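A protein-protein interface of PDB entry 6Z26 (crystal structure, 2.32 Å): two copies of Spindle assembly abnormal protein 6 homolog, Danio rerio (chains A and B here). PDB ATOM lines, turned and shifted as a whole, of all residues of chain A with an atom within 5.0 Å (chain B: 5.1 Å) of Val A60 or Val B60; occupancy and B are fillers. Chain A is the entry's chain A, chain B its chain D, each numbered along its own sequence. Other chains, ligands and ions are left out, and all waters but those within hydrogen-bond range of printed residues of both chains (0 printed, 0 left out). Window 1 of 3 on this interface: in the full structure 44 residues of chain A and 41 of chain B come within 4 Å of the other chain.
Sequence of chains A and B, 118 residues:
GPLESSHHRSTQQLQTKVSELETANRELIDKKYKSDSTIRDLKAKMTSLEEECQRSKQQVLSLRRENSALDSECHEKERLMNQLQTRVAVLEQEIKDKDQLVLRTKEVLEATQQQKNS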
ATOM      1  N   SER A  56      34.115   8.122 -23.467  1.00  0.00           N
ATOM      2  CA  SER A  56      32.837   8.026 -22.761  1.00  0.00           C
ATOM      3  C   SER A  56      32.293   6.609 -22.813  1.00  0.00           C
ATOM      4  O   SER A  56      31.696   6.188 -21.839  1.00  0.00           O
ATOM      5  CB  SER A  56      31.814   9.061 -23.222  1.00  0.00           C
ATOM      6  OG  SER A  56      31.855   9.290 -24.620  1.00  0.00           O
ATOM      7  N   LYS A  57      32.573   5.841 -23.891  1.00  0.00           N
ATOM      8  CA  LYS A  57      32.174   4.432 -24.000  1.00  0.00           C
ATOM      9  C   LYS A  57      32.813   3.622 -22.851  1.00  0.00           C
ATOM     10  O   LYS A  57      32.129   2.817 -22.225  1.00  0.00           O
ATOM     11  CB  LYS A  57      32.568   3.837 -25.368  1.00  0.00           C
ATOM     12  CG  LYS A  57      31.913   2.484 -25.651  1.00  0.00           C
ATOM     13  CD  LYS A  57      32.626   1.681 -26.738  1.00  0.00           C
ATOM     14  CE  LYS A  57      33.144   0.345 -26.236  1.00  0.00           C
ATOM     15  NZ  LYS A  57      32.065  -0.675 -26.043  1.00  0.00           N
ATOM     16  N   GLN A  58      34.104   3.855 -22.566  1.00  0.00           N
ATOM     17  CA  GLN A  58      34.810   3.175 -21.482  1.00  0.00           C
ATOM     18  C   GLN A  58      34.368   3.648 -20.101  1.00  0.00           C
ATOM     19  O   GLN A  58      34.370   2.857 -19.155  1.00  0.00           O
ATOM     20  CB  GLN A  58      36.331   3.261 -21.659  1.00  0.00           C
ATOM     21  CG  GLN A  58      36.880   2.298 -22.735  1.00  0.00           C
ATOM     22  CD  GLN A  58      36.419   0.855 -22.553  1.00  0.00           C
ATOM     23  OE1 GLN A  58      36.624   0.222 -21.503  1.00  0.00           O
ATOM     24  NE2 GLN A  58      35.767   0.306 -23.568  1.00  0.00           N
ATOM     25  N   GLN A  59      33.961   4.918 -19.999  1.00  0.00           N
ATOM     26  CA  GLN A  59      33.449   5.525 -18.791  1.00  0.00           C
ATOM     27  C   GLN A  59      32.061   4.905 -18.479  1.00  0.00           C
ATOM     28  O   GLN A  59      31.796   4.558 -17.321  1.00  0.00           O
ATOM     29  CB  GLN A  59      33.358   7.029 -19.042  1.00  0.00           C
ATOM     30  CG  GLN A  59      32.988   7.888 -17.852  1.00  0.00           C
ATOM     31  CD  GLN A  59      32.920   9.363 -18.189  1.00  0.00           C
ATOM     32  OE1 GLN A  59      33.418   9.847 -19.224  1.00  0.00           O
ATOM     33  NE2 GLN A  59      32.306  10.112 -17.288  1.00  0.00           N
ATOM     34  N   VAL A  60      31.202   4.715 -19.525  1.00  0.00           N
ATOM     35  CA  VAL A  60      29.874   4.090 -19.395  1.00  0.00           C
ATOM     36  C   VAL A  60      30.045   2.660 -18.893  1.00  0.00           C
ATOM     37  O   VAL A  60      29.390   2.285 -17.934  1.00  0.00           O
ATOM     38  CB  VAL A  60      29.035   4.131 -20.708  1.00  0.00           C
ATOM     39  CG1 VAL A  60      27.895   3.136 -20.668  1.00  0.00           C
ATOM     40  CG2 VAL A  60      28.513   5.527 -21.000  1.00  0.00           C
ATOM     41  N   LEU A  61      30.949   1.890 -19.520  1.00  0.00           N
ATOM     42  CA  LEU A  61      31.243   0.499 -19.178  1.00  0.00           C
ATOM     43  C   LEU A  61      31.754   0.342 -17.773  1.00  0.00           C
ATOM     44  O   LEU A  61      31.375  -0.607 -17.093  1.00  0.00           O
ATOM     45  CB  LEU A  61      32.211  -0.129 -20.201  1.00  0.00           C
ATOM     46  CG  LEU A  61      31.622  -0.319 -21.611  1.00  0.00           C
ATOM     47  CD1 LEU A  61      32.686  -0.600 -22.619  1.00  0.00           C
ATOM     48  CD2 LEU A  61      30.490  -1.362 -21.646  1.00  0.00           C
ATOM     49  N   SER A  62      32.563   1.303 -17.321  1.00  0.00           N
ATOM     50  CA  SER A  62      33.120   1.352 -15.973  1.00  0.00           C
ATOM     51  C   SER A  62      31.978   1.581 -14.963  1.00  0.00           C
ATOM     52  O   SER A  62      31.867   0.857 -13.969  1.00  0.00           O
ATOM     53  CB  SER A  62      34.181   2.443 -15.890  1.00  0.00           C
ATOM     54  OG  SER A  62      34.779   2.499 -14.610  1.00  0.00           O
ATOM     55  N   LEU A  63      31.093   2.540 -15.277  1.00  0.00           N
ATOM     56  CA  LEU A  63      29.932   2.893 -14.461  1.00  0.00           C
ATOM     57  C   LEU A  63      28.860   1.787 -14.436  1.00  0.00           C
ATOM     58  O   LEU A  63      28.140   1.680 -13.447  1.00  0.00           O
ATOM     59  CB  LEU A  63      29.343   4.225 -14.945  1.00  0.00           C
ATOM     60  CG  LEU A  63      30.076   5.506 -14.508  1.00  0.00           C
ATOM     61  CD1 LEU A  63      29.676   6.657 -15.370  1.00  0.00           C
ATOM     62  CD2 LEU A  63      29.776   5.860 -13.057  1.00  0.00           C
ATOM     63  N   ARG A  64      28.772   0.959 -15.497  1.00  0.00           N
ATOM     64  CA  ARG A  64      27.839  -0.175 -15.541  1.00  0.00           C
ATOM     65  C   ARG A  64      28.328  -1.326 -14.637  1.00  0.00           C
ATOM     66  O   ARG A  64      27.528  -1.977 -13.973  1.00  0.00           O
ATOM     67  CB  ARG A  64      27.617  -0.651 -16.968  1.00  0.00           C
ATOM     68  CG  ARG A  64      26.740   0.297 -17.753  1.00  0.00           C
ATOM     69  CD  ARG A  64      26.044  -0.354 -18.930  1.00  0.00           C
ATOM     70  NE  ARG A  64      24.740   0.285 -19.125  1.00  0.00           N
ATOM     71  CZ  ARG A  64      24.437   1.062 -20.150  1.00  0.00           C
ATOM     72  NH1 ARG A  64      25.309   1.222 -21.139  1.00  0.00           N
ATOM     73  NH2 ARG A  64      23.244   1.634 -20.234  1.00  0.00           N
ATOM     74  N   SER B  56      26.179   9.551 -25.018  1.00  0.00           N
ATOM     75  CA  SER B  56      27.012   8.882 -24.020  1.00  0.00           C
ATOM     76  C   SER B  56      27.303   9.782 -22.821  1.00  0.00           C
ATOM     77  O   SER B  56      27.393   9.272 -21.705  1.00  0.00           O
ATOM     78  CB  SER B  56      28.277   8.279 -24.622  1.00  0.00           C
ATOM     79  OG  SER B  56      28.885   9.106 -25.597  1.00  0.00           O
ATOM     80  N   LYS B  57      27.366  11.117 -23.027  1.00  0.00           N
ATOM     81  CA  LYS B  57      27.576  12.084 -21.940  1.00  0.00           C
ATOM     82  C   LYS B  57      26.390  12.016 -20.986  1.00  0.00           C
ATOM     83  O   LYS B  57      26.574  12.011 -19.765  1.00  0.00           O
ATOM     84  CB  LYS B  57      27.741  13.516 -22.482  1.00  0.00           C
ATOM     85  CG  LYS B  57      28.243  14.504 -21.425  1.00  0.00           C
ATOM     86  CD  LYS B  57      28.112  15.951 -21.864  1.00  0.00           C
ATOM     87  CE  LYS B  57      29.440  16.534 -22.295  1.00  0.00           C
ATOM     88  NZ  LYS B  57      29.294  17.906 -22.850  1.00  0.00           N
ATOM     89  N   GLN B  58      25.177  11.911 -21.551  1.00  0.00           N
ATOM     90  CA  GLN B  58      23.944  11.809 -20.778  1.00  0.00           C
ATOM     91  C   GLN B  58      23.815  10.450 -20.108  1.00  0.00           C
ATOM     92  O   GLN B  58      23.313  10.367 -18.992  1.00  0.00           O
ATOM     93  CB  GLN B  58      22.726  12.143 -21.643  1.00  0.00           C
ATOM     94  CG  GLN B  58      22.622  13.624 -21.992  1.00  0.00           C
ATOM     95  CD  GLN B  58      22.604  14.526 -20.777  1.00  0.00           C
ATOM     96  OE1 GLN B  58      21.692  14.473 -19.944  1.00  0.00           O
ATOM     97  NE2 GLN B  58      23.624  15.372 -20.649  1.00  0.00           N
ATOM     98  N   GLN B  59      24.308   9.405 -20.768  1.00  0.00           N
ATOM     99  CA  GLN B  59      24.322   8.045 -20.270  1.00  0.00           C
ATOM    100  C   GLN B  59      25.271   7.973 -19.056  1.00  0.00           C
ATOM    101  O   GLN B  59      24.898   7.369 -18.050  1.00  0.00           O
ATOM    102  CB  GLN B  59      24.776   7.140 -21.411  1.00  0.00           C
ATOM    103  CG  GLN B  59      24.706   5.664 -21.182  1.00  0.00           C
ATOM    104  CD  GLN B  59      25.135   4.858 -22.383  1.00  0.00           C
ATOM    105  OE1 GLN B  59      25.196   3.641 -22.302  1.00  0.00           O
ATOM    106  NE2 GLN B  59      25.408   5.488 -23.535  1.00  0.00           N
ATOM    107  N   VAL B  60      26.455   8.639 -19.127  1.00  0.00           N
ATOM    108  CA  VAL B  60      27.411   8.680 -18.016  1.00  0.00           C
ATOM    109  C   VAL B  60      26.784   9.364 -16.801  1.00  0.00           C
ATOM    110  O   VAL B  60      26.804   8.812 -15.701  1.00  0.00           O
ATOM    111  CB  VAL B  60      28.825   9.246 -18.356  1.00  0.00           C
ATOM    112  CG1 VAL B  60      29.600   8.342 -19.310  1.00  0.00           C
ATOM    113  CG2 VAL B  60      28.807  10.674 -18.860  1.00  0.00           C
ATOM    114  N   LEU B  61      26.175  10.537 -17.028  1.00  0.00           N
ATOM    115  CA  LEU B  61      25.522  11.339 -15.997  1.00  0.00           C
ATOM    116  C   LEU B  61      24.362  10.602 -15.361  1.00  0.00           C
ATOM    117  O   LEU B  61      24.164  10.713 -14.148  1.00  0.00           O
ATOM    118  CB  LEU B  61      25.075  12.695 -16.552  1.00  0.00           C
ATOM    119  CG  LEU B  61      26.220  13.637 -16.953  1.00  0.00           C
ATOM    120  CD1 LEU B  61      25.729  14.782 -17.856  1.00  0.00           C
ATOM    121  CD2 LEU B  61      26.962  14.156 -15.724  1.00  0.00           C
ATOM    122  N   SER B  62      23.624   9.820 -16.165  1.00  0.00           N
ATOM    123  CA  SER B  62      22.499   9.012 -15.706  1.00  0.00           C
ATOM    124  C   SER B  62      23.030   7.902 -14.794  1.00  0.00           C
ATOM    125  O   SER B  62      22.501   7.719 -13.696  1.00  0.00           O
ATOM    126  CB  SER B  62      21.743   8.428 -16.893  1.00  0.00           C
ATOM    127  OG  SER B  62      20.607   7.695 -16.470  1.00  0.00           O
ATOM    128  N   LEU B  63      24.114   7.224 -15.215  1.00  0.00           N
ATOM    129  CA  LEU B  63      24.778   6.164 -14.458  1.00  0.00           C
ATOM    130  C   LEU B  63      25.432   6.664 -13.161  1.00  0.00           C
ATOM    131  O   LEU B  63      25.504   5.911 -12.200  1.00  0.00           O
ATOM    132  CB  LEU B  63      25.803   5.437 -15.338  1.00  0.00           C
ATOM    133  CG  LEU B  63      25.242   4.402 -16.317  1.00  0.00           C
ATOM    134  CD1 LEU B  63      26.222   4.105 -17.412  1.00  0.00           C
ATOM    135  CD2 LEU B  63      24.912   3.103 -15.600  1.00  0.00           C
ATOM    136  N   ARG B  64      25.895   7.921 -13.131  1.00  0.00           N
ATOM    137  CA  ARG B  64      26.506   8.517 -11.946  1.00  0.00           C
ATOM    138  C   ARG B  64      25.437   8.815 -10.910  1.00  0.00           C
ATOM    139  O   ARG B  64      25.677   8.605  -9.722  1.00  0.00           O
ATOM    140  CB  ARG B  64      27.299   9.779 -12.306  1.00  0.00           C
ATOM    141  CG  ARG B  64      28.621   9.485 -12.989  1.00  0.00           C
ATOM    142  CD  ARG B  64      29.578  10.645 -12.830  1.00  0.00           C
ATOM    143  NE  ARG B  64      30.963  10.250 -13.084  1.00  0.00           N
ATOM    144  CZ  ARG B  64      31.703  10.721 -14.082  1.00  0.00           C
ATOM    145  NH1 ARG B  64      31.206  11.617 -14.925  1.00  0.00           N
ATOM    146  NH2 ARG B  64      32.952  10.299 -14.240  1.00  0.00           N
ATOM    147  N   ARG B  65      24.247   9.262 -11.365  1.00  0.00           N
ATOM    148  CA  ARG B  65      23.080   9.576 -10.538  1.00  0.00           C
ATOM    149  C   ARG B  65      22.539   8.282  -9.910  1.00  0.00           C
ATOM    150  O   ARG B  65      22.211   8.267  -8.712  1.00  0.00           O
ATOM    151  CB  ARG B  65      22.007  10.280 -11.384  1.00  0.00           C
ATOM    152  CG  ARG B  65      20.911  10.971 -10.575  1.00  0.00           C
ATOM    153  CD  ARG B  65      20.097  11.938 -11.426  1.00  0.00           C
ATOM    154  NE  ARG B  65      18.950  12.494 -10.682  1.00  0.00           N
ATOM    155  CZ  ARG B  65      18.294  13.596 -11.044  1.00  0.00           C
ATOM    156  NH1 ARG B  65      18.648  14.293 -12.108  1.00  0.00           N
ATOM    157  NH2 ARG B  65      17.261  14.016 -10.304  1.00  0.00           N
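Ser B56 touches its own counterpart, Ser A56.
Ser A56 touches Val B60, and with the chains exchanged Val A60 touches Ser B56.
Val A60 touches its own counterpart, Val B60.
Leu A63 touches Arg B64, and with the chains exchanged Arg A64 touches Leu B63.
Positions printed for both chains: 56, 57, 58, 59, 60, 61, 62, 63 and 64.
Of the 13 pairs that touch across the chains among the printed residues, 13 have their exchanged pair printed and touching as well.
Val B60 touches Ser A56.
Gln A59 touches Val B60.
Ser B56 touches Val A60.
OE1 of Gln B59 touches CG1 of Val A60, at 3.2 Å.
Val A60 touches Val B60.
Val A60 touches Leu B63.
Leu A63 touches Val B60 (CD1 to O, 3.6 Å).
Leu A63 touches Leu B63 (CB to CB, 3.8 Å).
CG of Arg B64 touches CD2 of Leu A63 (3.8 Å).
CD1 of Leu B63 touches CG of Arg A64, 3.9 Å away.
Of the 10 printed residues of chain B, 5 touch a printed residue of chain A.
Hydrophobic or aromatic side chains of chain B that line the printed part of chain A: Val B60 and Leu B63.
Among the printed residues, no Asp or Glu carboxylate lies within 4 Å of a Lys or Arg side-chain nitrogen of the other chain.
The side-chain hydroxyl (OG) of Ser A56 sits at hydrogen-bond distance from the side-chain hydroxyl (OG) of Ser B56, at 3.1 Å.
NH1 of Arg A64 is in hydrogen-bond range of OE1 of Gln B59, 2.7 Å away.
NE2 of Gln A59 lies close to NH1 of Arg B64 (3.0 Å).
Val A60 touches just these residues of chain B: Ser B56, Gln B59, Val B60 and Leu B63.
Of the printed residues of chain A, Ser B56 touches Ser A56 and Val A60.
Lys B57 touches none of the printed residues of chain A.
Of chain A, only Ser A56, Gln A59, Val A60 and Leu A63 come within 4 Å of Val B60.
Ser B62 touches none of the printed residues of chain A.
Of the printed residues of chain A, Leu B63 touches Val A60 (3.7 Å), Leu A63 (3.8 Å) and Arg A64 (3.9 Å).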
